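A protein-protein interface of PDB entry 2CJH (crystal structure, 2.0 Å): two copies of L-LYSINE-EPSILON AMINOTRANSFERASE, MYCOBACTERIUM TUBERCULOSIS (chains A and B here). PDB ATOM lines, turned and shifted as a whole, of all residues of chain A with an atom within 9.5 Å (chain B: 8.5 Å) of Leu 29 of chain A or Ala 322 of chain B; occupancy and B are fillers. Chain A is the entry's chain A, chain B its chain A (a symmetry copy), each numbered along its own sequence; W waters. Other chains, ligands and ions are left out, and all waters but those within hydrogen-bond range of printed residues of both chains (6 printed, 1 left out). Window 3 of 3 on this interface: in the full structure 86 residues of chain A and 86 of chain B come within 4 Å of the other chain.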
ATOM      1  N   HIS A  21      -7.351  11.668 -16.738  1.00  0.00           N
ATOM      2  CA  HIS A  21      -8.661  12.239 -17.020  1.00  0.00           C
ATOM      3  C   HIS A  21      -9.178  13.096 -15.873  1.00  0.00           C
ATOM      4  O   HIS A  21      -9.763  14.154 -16.114  1.00  0.00           O
ATOM      5  CB  HIS A  21      -9.677  11.146 -17.365  1.00  0.00           C
ATOM      6  CG  HIS A  21      -9.435  10.529 -18.705  1.00  0.00           C
ATOM      7  ND1 HIS A  21     -10.246  10.769 -19.794  1.00  0.00           N
ATOM      8  CD2 HIS A  21      -8.438   9.722 -19.141  1.00  0.00           C
ATOM      9  CE1 HIS A  21      -9.771  10.113 -20.843  1.00  0.00           C
ATOM     10  NE2 HIS A  21      -8.676   9.472 -20.473  1.00  0.00           N
ATOM     11  N   VAL A  23      -7.228  14.719 -13.580  1.00  0.00           N
ATOM     12  CA  VAL A  23      -6.405  15.942 -13.515  1.00  0.00           C
ATOM     13  C   VAL A  23      -6.831  16.945 -14.579  1.00  0.00           C
ATOM     14  O   VAL A  23      -7.022  18.113 -14.286  1.00  0.00           O
ATOM     15  CB  VAL A  23      -4.879  15.640 -13.619  1.00  0.00           C
ATOM     16  CG1 VAL A  23      -4.049  16.935 -13.702  1.00  0.00           C
ATOM     17  CG2 VAL A  23      -4.427  14.809 -12.421  1.00  0.00           C
ATOM     18  N   LEU A  24      -7.023  16.485 -15.807  1.00  0.00           N
ATOM     19  CA  LEU A  24      -7.387  17.385 -16.882  1.00  0.00           C
ATOM     20  C   LEU A  24      -8.785  17.944 -16.662  1.00  0.00           C
ATOM     21  O   LEU A  24      -9.055  19.117 -16.989  1.00  0.00           O
ATOM     22  CB  LEU A  24      -7.330  16.657 -18.228  1.00  0.00           C
ATOM     23  CG  LEU A  24      -5.942  16.220 -18.712  1.00  0.00           C
ATOM     24  CD1 LEU A  24      -6.119  15.321 -19.916  1.00  0.00           C
ATOM     25  CD2 LEU A  24      -5.045  17.397 -19.030  1.00  0.00           C
ATOM     26  N   GLY A  25      -9.677  17.096 -16.144  1.00  0.00           N
ATOM     27  CA  GLY A  25     -11.098  17.443 -15.984  1.00  0.00           C
ATOM     28  C   GLY A  25     -11.334  18.583 -15.011  1.00  0.00           C
ATOM     29  O   GLY A  25     -12.382  19.215 -15.038  1.00  0.00           O
ATOM     30  N   ARG A  26     -10.366  18.849 -14.155  1.00  0.00           N
ATOM     31  CA  ARG A  26     -10.421  20.024 -13.276  1.00  0.00           C
ATOM     32  C   ARG A  26     -10.282  21.353 -14.058  1.00  0.00           C
ATOM     33  O   ARG A  26     -10.716  22.386 -13.568  1.00  0.00           O
ATOM     34  CB  ARG A  26      -9.335  19.958 -12.198  1.00  0.00           C
ATOM     35  CG  ARG A  26      -9.374  18.708 -11.307  1.00  0.00           C
ATOM     36  CD  ARG A  26      -8.353  18.875 -10.171  1.00  0.00           C
ATOM     37  NE  ARG A  26      -7.833  17.603  -9.624  1.00  0.00           N
ATOM     38  CZ  ARG A  26      -6.533  17.285  -9.517  1.00  0.00           C
ATOM     39  NH1 ARG A  26      -5.575  18.132  -9.927  1.00  0.00           N
ATOM     40  NH2 ARG A  26      -6.184  16.112  -8.992  1.00  0.00           N
ATOM     41  N   SER A  27      -9.694  21.313 -15.265  1.00  0.00           N
ATOM     42  CA  SER A  27      -9.377  22.526 -16.010  1.00  0.00           C
ATOM     43  C   SER A  27     -10.049  22.604 -17.375  1.00  0.00           C
ATOM     44  O   SER A  27     -10.146  23.683 -17.948  1.00  0.00           O
ATOM     45  CB  SER A  27      -7.865  22.614 -16.227  1.00  0.00           C
ATOM     46  OG  SER A  27      -7.197  22.737 -15.010  1.00  0.00           O
ATOM     47  N   MET A  28     -10.493  21.466 -17.910  1.00  0.00           N
ATOM     48  CA  MET A  28     -10.967  21.433 -19.278  1.00  0.00           C
ATOM     49  C   MET A  28     -12.146  20.512 -19.427  1.00  0.00           C
ATOM     50  O   MET A  28     -12.393  19.665 -18.588  1.00  0.00           O
ATOM     51  CB  MET A  28      -9.868  20.937 -20.241  1.00  0.00           C
ATOM     52  CG  MET A  28      -8.421  21.065 -19.748  1.00  0.00           C
ATOM     53  SD  MET A  28      -7.164  20.684 -21.024  1.00  0.00           S
ATOM     54  CE  MET A  28      -8.090  19.472 -21.941  1.00  0.00           C
ATOM     55  N   LEU A  29     -12.850  20.680 -20.537  1.00  0.00           N
ATOM     56  CA  LEU A  29     -13.813  19.709 -20.994  1.00  0.00           C
ATOM     57  C   LEU A  29     -13.088  18.442 -21.459  1.00  0.00           C
ATOM     58  O   LEU A  29     -12.245  18.497 -22.357  1.00  0.00           O
ATOM     59  CB  LEU A  29     -14.633  20.330 -22.140  1.00  0.00           C
ATOM     60  CG  LEU A  29     -16.055  19.827 -22.295  1.00  0.00           C
ATOM     61  CD1 LEU A  29     -16.737  19.853 -20.950  1.00  0.00           C
ATOM     62  CD2 LEU A  29     -16.745  20.720 -23.267  1.00  0.00           C
ATOM     63  N   VAL A  30     -13.388  17.311 -20.846  1.00  0.00           N
ATOM     64  CA  VAL A  30     -12.667  16.077 -21.182  1.00  0.00           C
ATOM     65  C   VAL A  30     -13.518  15.161 -22.087  1.00  0.00           C
ATOM     66  O   VAL A  30     -14.138  14.202 -21.622  1.00  0.00           O
ATOM     67  CB  VAL A  30     -12.128  15.361 -19.898  1.00  0.00           C
ATOM     68  CG1 VAL A  30     -11.791  13.905 -20.176  1.00  0.00           C
ATOM     69  CG2 VAL A  30     -10.896  16.087 -19.385  1.00  0.00           C
ATOM     70  N   ASP A  31     -13.558  15.468 -23.375  1.00  0.00           N
ATOM     71  CA  ASP A  31     -14.480  14.774 -24.285  1.00  0.00           C
ATOM     72  C   ASP A  31     -13.790  13.866 -25.337  1.00  0.00           C
ATOM     73  O   ASP A  31     -14.438  13.370 -26.266  1.00  0.00           O
ATOM     74  CB  ASP A  31     -15.411  15.796 -24.958  1.00  0.00           C
ATOM     75  CG  ASP A  31     -14.651  16.796 -25.837  1.00  0.00           C
ATOM     76  OD1 ASP A  31     -13.458  17.095 -25.557  1.00  0.00           O
ATOM     77  OD2 ASP A  31     -15.255  17.275 -26.829  1.00  0.00           O
ATOM     78  N   GLY A  32     -12.488  13.633 -25.185  1.00  0.00           N
ATOM     79  CA  GLY A  32     -11.767  12.815 -26.154  1.00  0.00           C
ATOM     80  C   GLY A  32     -11.870  11.331 -25.864  1.00  0.00           C
ATOM     81  O   GLY A  32     -12.765  10.888 -25.136  1.00  0.00           O
ATOM     82  N   LEU A  33     -10.936  10.568 -26.420  1.00  0.00           N
ATOM     83  CA  LEU A  33     -10.956   9.113 -26.292  1.00  0.00           C
ATOM     84  C   LEU A  33     -10.708   8.630 -24.860  1.00  0.00           C
ATOM     85  O   LEU A  33      -9.994   9.271 -24.077  1.00  0.00           O
ATOM     86  CB  LEU A  33      -9.968   8.459 -27.262  1.00  0.00           C
ATOM     87  CG  LEU A  33     -10.153   8.701 -28.755  1.00  0.00           C
ATOM     88  CD1 LEU A  33      -8.972   8.116 -29.506  1.00  0.00           C
ATOM     89  CD2 LEU A  33     -11.444   8.078 -29.228  1.00  0.00           C
ATOM     90  N   ASN B  95      -3.816  16.429 -29.088  1.00  0.00           N
ATOM     91  CA  ASN B  95      -4.197  16.495 -27.679  1.00  0.00           C
ATOM     92  C   ASN B  95      -5.670  16.846 -27.451  1.00  0.00           C
ATOM     93  O   ASN B  95      -6.176  16.680 -26.334  1.00  0.00           O
ATOM     94  CB  ASN B  95      -3.326  17.513 -26.931  1.00  0.00           C
ATOM     95  CG  ASN B  95      -1.855  17.302 -27.178  1.00  0.00           C
ATOM     96  OD1 ASN B  95      -1.306  16.199 -26.948  1.00  0.00           O
ATOM     97  ND2 ASN B  95      -1.192  18.350 -27.664  1.00  0.00           N
ATOM     98  N   SER B  96      -6.327  17.350 -28.500  1.00  0.00           N
ATOM     99  CA  SER B  96      -7.776  17.596 -28.525  1.00  0.00           C
ATOM    100  C   SER B  96      -8.539  16.323 -28.178  1.00  0.00           C
ATOM    101  O   SER B  96      -9.550  16.383 -27.494  1.00  0.00           O
ATOM    102  CB  SER B  96      -8.207  18.002 -29.943  1.00  0.00           C
ATOM    103  OG  SER B  96      -7.663  19.247 -30.318  1.00  0.00           O
ATOM    104  N   ASP B  97      -8.045  15.185 -28.687  1.00  0.00           N
ATOM    105  CA  ASP B  97      -8.765  13.891 -28.694  1.00  0.00           C
ATOM    106  C   ASP B  97      -8.076  12.841 -27.852  1.00  0.00           C
ATOM    107  O   ASP B  97      -8.711  11.894 -27.402  1.00  0.00           O
ATOM    108  CB  ASP B  97      -8.759  13.214 -30.093  1.00  0.00           C
ATOM    109  CG  ASP B  97      -8.965  14.154 -31.217  1.00  0.00           C
ATOM    110  OD1 ASP B  97     -10.101  14.645 -31.385  1.00  0.00           O
ATOM    111  OD2 ASP B  97      -7.971  14.393 -31.938  1.00  0.00           O
ATOM    112  N   TYR B  99      -5.364  12.010 -24.821  1.00  0.00           N
ATOM    113  CA  TYR B  99      -4.658  12.496 -23.640  1.00  0.00           C
ATOM    114  C   TYR B  99      -3.451  11.638 -23.288  1.00  0.00           C
ATOM    115  O   TYR B  99      -3.383  10.461 -23.666  1.00  0.00           O
ATOM    116  CB  TYR B  99      -5.615  12.630 -22.446  1.00  0.00           C
ATOM    117  CG  TYR B  99      -6.893  13.317 -22.834  1.00  0.00           C
ATOM    118  CD1 TYR B  99      -6.872  14.522 -23.549  1.00  0.00           C
ATOM    119  CD2 TYR B  99      -8.118  12.761 -22.522  1.00  0.00           C
ATOM    120  CE1 TYR B  99      -8.053  15.148 -23.949  1.00  0.00           C
ATOM    121  CE2 TYR B  99      -9.298  13.376 -22.905  1.00  0.00           C
ATOM    122  CZ  TYR B  99      -9.255  14.563 -23.613  1.00  0.00           C
ATOM    123  OH  TYR B  99     -10.431  15.170 -23.968  1.00  0.00           O
ATOM    124  N   MET B 103       0.910  15.569 -21.149  1.00  0.00           N
ATOM    125  CA  MET B 103      -0.056  16.641 -21.208  1.00  0.00           C
ATOM    126  C   MET B 103      -0.619  16.970 -19.821  1.00  0.00           C
ATOM    127  O   MET B 103      -0.653  18.140 -19.439  1.00  0.00           O
ATOM    128  CB  MET B 103      -1.192  16.298 -22.175  1.00  0.00           C
ATOM    129  CG  MET B 103      -2.291  17.364 -22.248  1.00  0.00           C
ATOM    130  SD  MET B 103      -3.636  16.738 -23.267  1.00  0.00           S
ATOM    131  CE  MET B 103      -4.836  18.044 -23.105  1.00  0.00           C
ATOM    132  N   PRO B 120     -10.766  29.153 -13.750  1.00  0.00           N
ATOM    133  CA  PRO B 120     -10.346  27.758 -13.756  1.00  0.00           C
ATOM    134  C   PRO B 120     -10.371  27.060 -15.133  1.00  0.00           C
ATOM    135  O   PRO B 120      -9.783  25.987 -15.248  1.00  0.00           O
ATOM    136  CB  PRO B 120     -11.391  27.090 -12.862  1.00  0.00           C
ATOM    137  CG  PRO B 120     -12.644  27.852 -13.178  1.00  0.00           C
ATOM    138  CD  PRO B 120     -12.162  29.297 -13.289  1.00  0.00           C
ATOM    139  N   HIS B 121     -11.055  27.618 -16.123  1.00  0.00           N
ATOM    140  CA  HIS B 121     -11.181  26.981 -17.449  1.00  0.00           C
ATOM    141  C   HIS B 121      -9.959  27.294 -18.278  1.00  0.00           C
ATOM    142  O   HIS B 121      -9.660  28.471 -18.534  1.00  0.00           O
ATOM    143  CB  HIS B 121     -12.400  27.490 -18.204  1.00  0.00           C
ATOM    144  CG  HIS B 121     -13.656  27.437 -17.404  1.00  0.00           C
ATOM    145  ND1 HIS B 121     -14.243  26.248 -17.033  1.00  0.00           N
ATOM    146  CD2 HIS B 121     -14.399  28.419 -16.842  1.00  0.00           C
ATOM    147  CE1 HIS B 121     -15.320  26.496 -16.311  1.00  0.00           C
ATOM    148  NE2 HIS B 121     -15.432  27.806 -16.173  1.00  0.00           N
ATOM    149  N   LEU B 122      -9.285  26.245 -18.713  1.00  0.00           N
ATOM    150  CA  LEU B 122      -8.076  26.394 -19.503  1.00  0.00           C
ATOM    151  C   LEU B 122      -8.350  25.841 -20.879  1.00  0.00           C
ATOM    152  O   LEU B 122      -9.069  24.828 -21.025  1.00  0.00           O
ATOM    153  CB  LEU B 122      -6.937  25.614 -18.829  1.00  0.00           C
ATOM    154  CG  LEU B 122      -5.970  26.330 -17.873  1.00  0.00           C
ATOM    155  CD1 LEU B 122      -6.422  27.621 -17.247  1.00  0.00           C
ATOM    156  CD2 LEU B 122      -5.299  25.399 -16.876  1.00  0.00           C
ATOM    157  N   PHE B 123      -7.782  26.491 -21.894  1.00  0.00           N
ATOM    158  CA  PHE B 123      -7.891  26.009 -23.273  1.00  0.00           C
ATOM    159  C   PHE B 123      -6.592  26.347 -24.004  1.00  0.00           C
ATOM    160  O   PHE B 123      -6.120  27.468 -23.906  1.00  0.00           O
ATOM    161  CB  PHE B 123      -9.079  26.682 -23.973  1.00  0.00           C
ATOM    162  CG  PHE B 123      -9.251  26.261 -25.401  1.00  0.00           C
ATOM    163  CD1 PHE B 123      -9.921  25.075 -25.716  1.00  0.00           C
ATOM    164  CD2 PHE B 123      -8.757  27.049 -26.435  1.00  0.00           C
ATOM    165  CE1 PHE B 123     -10.078  24.687 -27.048  1.00  0.00           C
ATOM    166  CE2 PHE B 123      -8.897  26.670 -27.756  1.00  0.00           C
ATOM    167  CZ  PHE B 123      -9.569  25.498 -28.067  1.00  0.00           C
ATOM    168  N   ASP B 141     -20.121  34.164 -27.855  1.00  0.00           N
ATOM    169  CA  ASP B 141     -21.075  33.134 -27.493  1.00  0.00           C
ATOM    170  C   ASP B 141     -21.752  33.511 -26.153  1.00  0.00           C
ATOM    171  O   ASP B 141     -22.971  33.371 -25.978  1.00  0.00           O
ATOM    172  CB  ASP B 141     -20.346  31.799 -27.357  1.00  0.00           C
ATOM    173  CG  ASP B 141     -21.227  30.714 -26.738  1.00  0.00           C
ATOM    174  OD1 ASP B 141     -21.967  30.016 -27.492  1.00  0.00           O
ATOM    175  OD2 ASP B 141     -21.146  30.556 -25.489  1.00  0.00           O
ATOM    176  N   VAL B 313     -17.916  34.475 -16.946  1.00  0.00           N
ATOM    177  CA  VAL B 313     -18.146  33.447 -17.991  1.00  0.00           C
ATOM    178  C   VAL B 313     -19.051  32.333 -17.464  1.00  0.00           C
ATOM    179  O   VAL B 313     -19.940  31.836 -18.171  1.00  0.00           O
ATOM    180  CB  VAL B 313     -16.797  32.844 -18.540  1.00  0.00           C
ATOM    181  CG1 VAL B 313     -17.049  31.601 -19.425  1.00  0.00           C
ATOM    182  CG2 VAL B 313     -15.987  33.906 -19.275  1.00  0.00           C
ATOM    183  N   ASP B 314     -18.823  31.948 -16.215  1.00  0.00           N
ATOM    184  CA  ASP B 314     -19.583  30.857 -15.600  1.00  0.00           C
ATOM    185  C   ASP B 314     -21.076  31.145 -15.370  1.00  0.00           C
ATOM    186  O   ASP B 314     -21.820  30.232 -15.092  1.00  0.00           O
ATOM    187  CB  ASP B 314     -18.909  30.418 -14.294  1.00  0.00           C
ATOM    188  CG  ASP B 314     -17.568  29.710 -14.539  1.00  0.00           C
ATOM    189  OD1 ASP B 314     -17.559  28.555 -14.967  1.00  0.00           O
ATOM    190  OD2 ASP B 314     -16.522  30.303 -14.308  1.00  0.00           O
ATOM    191  N   VAL B 316     -23.197  31.903 -17.570  1.00  0.00           N
ATOM    192  CA  VAL B 316     -23.923  31.344 -18.708  1.00  0.00           C
ATOM    193  C   VAL B 316     -23.517  29.862 -18.652  1.00  0.00           C
ATOM    194  O   VAL B 316     -22.368  29.520 -18.936  1.00  0.00           O
ATOM    195  CB  VAL B 316     -23.521  32.055 -20.051  1.00  0.00           C
ATOM    196  CG1 VAL B 316     -23.938  31.256 -21.271  1.00  0.00           C
ATOM    197  CG2 VAL B 316     -24.079  33.499 -20.089  1.00  0.00           C
ATOM    198  N   ALA B 317     -24.434  28.999 -18.240  1.00  0.00           N
ATOM    199  CA  ALA B 317     -24.085  27.606 -17.951  1.00  0.00           C
ATOM    200  C   ALA B 317     -23.619  26.814 -19.184  1.00  0.00           C
ATOM    201  O   ALA B 317     -22.893  25.838 -19.016  1.00  0.00           O
ATOM    202  CB  ALA B 317     -25.271  26.876 -17.298  1.00  0.00           C
ATOM    203  N   ASP B 318     -24.114  27.191 -20.371  1.00  0.00           N
ATOM    204  CA  ASP B 318     -23.800  26.497 -21.634  1.00  0.00           C
ATOM    205  C   ASP B 318     -22.787  27.313 -22.459  1.00  0.00           C
ATOM    206  O   ASP B 318     -22.901  27.418 -23.659  1.00  0.00           O
ATOM    207  CB  ASP B 318     -25.072  26.131 -22.428  1.00  0.00           C
ATOM    208  CG  ASP B 318     -26.114  27.271 -22.472  1.00  0.00           C
ATOM    209  OD1 ASP B 318     -25.916  28.325 -21.838  1.00  0.00           O
ATOM    210  OD2 ASP B 318     -27.161  27.105 -23.129  1.00  0.00           O
ATOM    211  N   ASN B 319     -21.775  27.856 -21.783  1.00  0.00           N
ATOM    212  CA  ASN B 319     -20.710  28.607 -22.428  1.00  0.00           C
ATOM    213  C   ASN B 319     -19.748  27.624 -23.176  1.00  0.00           C
ATOM    214  O   ASN B 319     -19.887  26.382 -23.076  1.00  0.00           O
ATOM    215  CB  ASN B 319     -19.982  29.460 -21.367  1.00  0.00           C
ATOM    216  CG  ASN B 319     -19.236  28.612 -20.339  1.00  0.00           C
ATOM    217  OD1 ASN B 319     -18.250  27.967 -20.674  1.00  0.00           O
ATOM    218  ND2 ASN B 319     -19.724  28.575 -19.096  1.00  0.00           N
ATOM    219  N   VAL B 320     -18.773  28.163 -23.907  1.00  0.00           N
ATOM    220  CA  VAL B 320     -17.933  27.343 -24.808  1.00  0.00           C
ATOM    221  C   VAL B 320     -17.015  26.408 -24.076  1.00  0.00           C
ATOM    222  O   VAL B 320     -16.460  25.511 -24.696  1.00  0.00           O
ATOM    223  CB  VAL B 320     -17.106  28.191 -25.831  1.00  0.00           C
ATOM    224  CG1 VAL B 320     -18.032  28.944 -26.744  1.00  0.00           C
ATOM    225  CG2 VAL B 320     -16.165  29.143 -25.113  1.00  0.00           C
ATOM    226  N   PHE B 321     -16.829  26.609 -22.772  1.00  0.00           N
ATOM    227  CA  PHE B 321     -15.986  25.721 -21.956  1.00  0.00           C
ATOM    228  C   PHE B 321     -16.762  24.558 -21.378  1.00  0.00           C
ATOM    229  O   PHE B 321     -16.182  23.597 -20.925  1.00  0.00           O
ATOM    230  CB  PHE B 321     -15.252  26.513 -20.868  1.00  0.00           C
ATOM    231  CG  PHE B 321     -14.486  27.673 -21.427  1.00  0.00           C
ATOM    232  CD1 PHE B 321     -13.265  27.461 -22.072  1.00  0.00           C
ATOM    233  CD2 PHE B 321     -15.010  28.953 -21.398  1.00  0.00           C
ATOM    234  CE1 PHE B 321     -12.583  28.520 -22.634  1.00  0.00           C
ATOM    235  CE2 PHE B 321     -14.331  30.028 -21.962  1.00  0.00           C
ATOM    236  CZ  PHE B 321     -13.125  29.810 -22.586  1.00  0.00           C
ATOM    237  N   ALA B 322     -18.082  24.641 -21.458  1.00  0.00           N
ATOM    238  CA  ALA B 322     -18.992  23.642 -20.895  1.00  0.00           C
ATOM    239  C   ALA B 322     -19.635  22.753 -21.986  1.00  0.00           C
ATOM    240  O   ALA B 322     -20.132  21.687 -21.691  1.00  0.00           O
ATOM    241  CB  ALA B 322     -20.081  24.361 -20.078  1.00  0.00           C
ATOM    242  N   VAL B 323     -19.615  23.187 -23.237  1.00  0.00           N
ATOM    243  CA  VAL B 323     -20.301  22.521 -24.351  1.00  0.00           C
ATOM    244  C   VAL B 323     -19.267  21.977 -25.361  1.00  0.00           C
ATOM    245  O   VAL B 323     -18.477  22.748 -25.909  1.00  0.00           O
ATOM    246  CB  VAL B 323     -21.275  23.498 -25.097  1.00  0.00           C
ATOM    247  CG1 VAL B 323     -21.815  22.879 -26.422  1.00  0.00           C
ATOM    248  CG2 VAL B 323     -22.442  23.927 -24.182  1.00  0.00           C
ATOM    249  N   PRO B 324     -19.325  20.673 -25.671  1.00  0.00           N
ATOM    250  CA  PRO B 324     -18.343  20.078 -26.582  1.00  0.00           C
ATOM    251  C   PRO B 324     -18.379  20.707 -27.975  1.00  0.00           C
ATOM    252  O   PRO B 324     -19.457  21.059 -28.485  1.00  0.00           O
ATOM    253  CB  PRO B 324     -18.795  18.616 -26.700  1.00  0.00           C
ATOM    254  CG  PRO B 324     -19.692  18.389 -25.555  1.00  0.00           C
ATOM    255  CD  PRO B 324     -20.358  19.700 -25.270  1.00  0.00           C
ATOM    256  N   SER B 325     -17.181  20.866 -28.536  1.00  0.00           N
ATOM    257  CA  SER B 325     -16.971  21.167 -29.952  1.00  0.00           C
ATOM    258  C   SER B 325     -17.228  22.611 -30.363  1.00  0.00           C
ATOM    259  O   SER B 325     -17.211  22.898 -31.547  1.00  0.00           O
ATOM    260  CB  SER B 325     -17.753  20.183 -30.854  1.00  0.00           C
ATOM    261  OG  SER B 325     -16.943  19.783 -31.982  1.00  0.00           O
ATOM    262  N   ARG B 326     -17.450  23.523 -29.402  1.00  0.00           N
ATOM    263  CA  ARG B 326     -17.604  24.949 -29.746  1.00  0.00           C
ATOM    264  C   ARG B 326     -16.241  25.591 -30.053  1.00  0.00           C
ATOM    265  O   ARG B 326     -16.157  26.461 -30.929  1.00  0.00           O
ATOM    266  CB  ARG B 326     -18.316  25.726 -28.621  1.00  0.00           C
ATOM    267  CG  ARG B 326     -19.751  25.254 -28.358  1.00  0.00           C
ATOM    268  CD  ARG B 326     -20.657  25.746 -29.428  1.00  0.00           C
ATOM    269  NE  ARG B 326     -20.891  27.174 -29.310  1.00  0.00           N
ATOM    270  CZ  ARG B 326     -21.023  28.006 -30.341  1.00  0.00           C
ATOM    271  NH1 ARG B 326     -20.909  27.555 -31.599  1.00  0.00           N
ATOM    272  NH2 ARG B 326     -21.257  29.292 -30.120  1.00  0.00           N
ATOM    273  N   LEU B 327     -15.214  25.193 -29.288  1.00  0.00           N
ATOM    274  CA  LEU B 327     -13.812  25.550 -29.555  1.00  0.00           C
ATOM    275  C   LEU B 327     -13.002  24.304 -29.892  1.00  0.00           C
ATOM    276  O   LEU B 327     -13.191  23.235 -29.301  1.00  0.00           O
ATOM    277  CB  LEU B 327     -13.126  26.272 -28.375  1.00  0.00           C
ATOM    278  CG  LEU B 327     -13.786  27.440 -27.633  1.00  0.00           C
ATOM    279  CD1 LEU B 327     -12.891  27.869 -26.457  1.00  0.00           C
ATOM    280  CD2 LEU B 327     -14.079  28.616 -28.567  1.00  0.00           C
HETATM  281  O   HOH W   1     -13.386  23.974 -18.331  1.00  0.00           O
HETATM  282  O   HOH W   2      -7.541  25.162 -13.839  1.00  0.00           O
HETATM  283  O   HOH W   3      -7.350  10.155 -24.565  1.00  0.00           O
HETATM  284  O   HOH W   4     -12.739  23.969 -15.250  1.00  0.00           O
HETATM  285  O   HOH W   5     -11.879  24.827 -20.376  1.00  0.00           O
HETATM  286  O   HOH W   6     -14.827  19.893 -27.522  1.00  0.00           O
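NE2 of His 121 of chain B lies within hydrogen-bond range of OD1 of Asp 314 of chain B (2.6 Å). The side-chain amide oxygen (OD1) of Asn 319 of chain B sits at hydrogen-bond distance from the backbone NH (N) of Phe 321 of chain B (2.9 Å). The side-chain amide oxygen (OD1) of Asn 319 of chain B is in hydrogen-bond range of the backbone NH (N) of Ala 322 of chain B (3.4 Å).
Arg 26 of chain A touches none of the printed residues of chain B. Leu 29 of chain A touches just these residues of chain B: Phe 321, Ala 322, Val 323 and Pro 324. Of the printed residues of chain B, Gly 32 of chain A touches Asp 97 and Tyr 99. Printed residues of chain B within 4 Å of Leu 33 of chain A: Asp 97. Printed residues of chain A within 4 Å of His 121 of chain B: Ser 27 (3.5 Å). Phe 123 of chain B touches none of the printed residues of chain A. Of the printed residues of chain A, Phe 321 of chain B touches Leu 29. Printed residues of chain A within 4 Å of Ala 322 of chain B: Leu 29. The nearest printed residue of chain A that does not touch His 121 of chain B is Met 28 of chain A (5.6 Å).
Among the printed residues, merely in contact across the chains: His 21 of chain A with Tyr 99 of chain B (3.5 Å), Leu 24 of chain A with Tyr 99 of chain B (3.6 Å), Ser 27 of chain A with Pro 120 of chain B (3.6 Å), Ser 27 of chain A with His 121 of chain B (3.5 Å), Met 28 of chain A with Met 103 of chain B (3.7 Å), Leu 29 of chain A with Phe 321 of chain B (3.8 Å), Leu 29 of chain A with Ala 322 of chain B (3.8 Å), Leu 29 of chain A with Val 323 of chain B (3.5 Å), Leu 29 of chain A with Pro 324 of chain B (3.5 Å), Val 30 of chain A with Tyr 99 of chain B (3.6 Å), Asp 31 of chain A with Pro 324 of chain B (3.8 Å) and Gly 32 of chain A with Asp 97 of chain B (3.4 Å).
No position is printed for both chains. Of the 16 pairs that touch across the chains among the printed residues, none has its exchanged pair printed and touching as well.
Water W2 lies within hydrogen-bond range of OG of Ser 27 of chain A (2.7 Å) and O of Pro 120 of chain B (2.8 Å). Water W3 lies within hydrogen-bond range of the backbone NH (N) of Tyr 99 of chain B and the backbone carbonyl oxygen (O) of Leu 33 of chain A. Water W6 lies within hydrogen-bond range of the side-chain carboxylate (OD2) of Asp 31 of chain A and the backbone NH (N) of Ser 325 of chain B. Water W1 bridges a ring nitrogen (ND1) of His 121 of chain B (2.8 Å) and the backbone carbonyl oxygen (O) of Ser 27 of chain A (3.3 Å). Water W5 lies within hydrogen-bond range of the backbone carbonyl oxygen (O) of Leu 122 of chain B (2.9 Å) and the backbone carbonyl oxygen (O) of Ser 27 of chain A (3.2 Å). Water W4 lies within hydrogen-bond range of the backbone carbonyl oxygen of Arg 26 of chain A (3.1 Å) and a ring nitrogen (ND1) of His 121 of chain B (3.3 Å).
Hydrophobic or aromatic side chains of chain A that line the printed part of chain B: His 21, Leu 24, Met 28, Leu 29, Val 30 and Leu 33. Along chain B the printed residues that touch a printed residue of chain A span positions 97 to 324. Among the printed residues, 16 pairs touch across the chains.
The backbone carbonyl oxygen of Ser 27 of chain A lies within hydrogen-bond range of the backbone NH of Leu 122 of chain B. The backbone NH of Asp 31 of chain A sits at hydrogen-bond distance from the side-chain hydroxyl of Tyr 99 of chain B (3.2 Å). OH of Tyr 99 of chain B sits at hydrogen-bond distance from N of Gly 32 of chain A (2.8 Å). The backbone carbonyl oxygen (O) of Asp 97 of chain B sits at hydrogen-bond distance from the backbone NH (N) of Leu 33 of chain A (2.8 Å).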
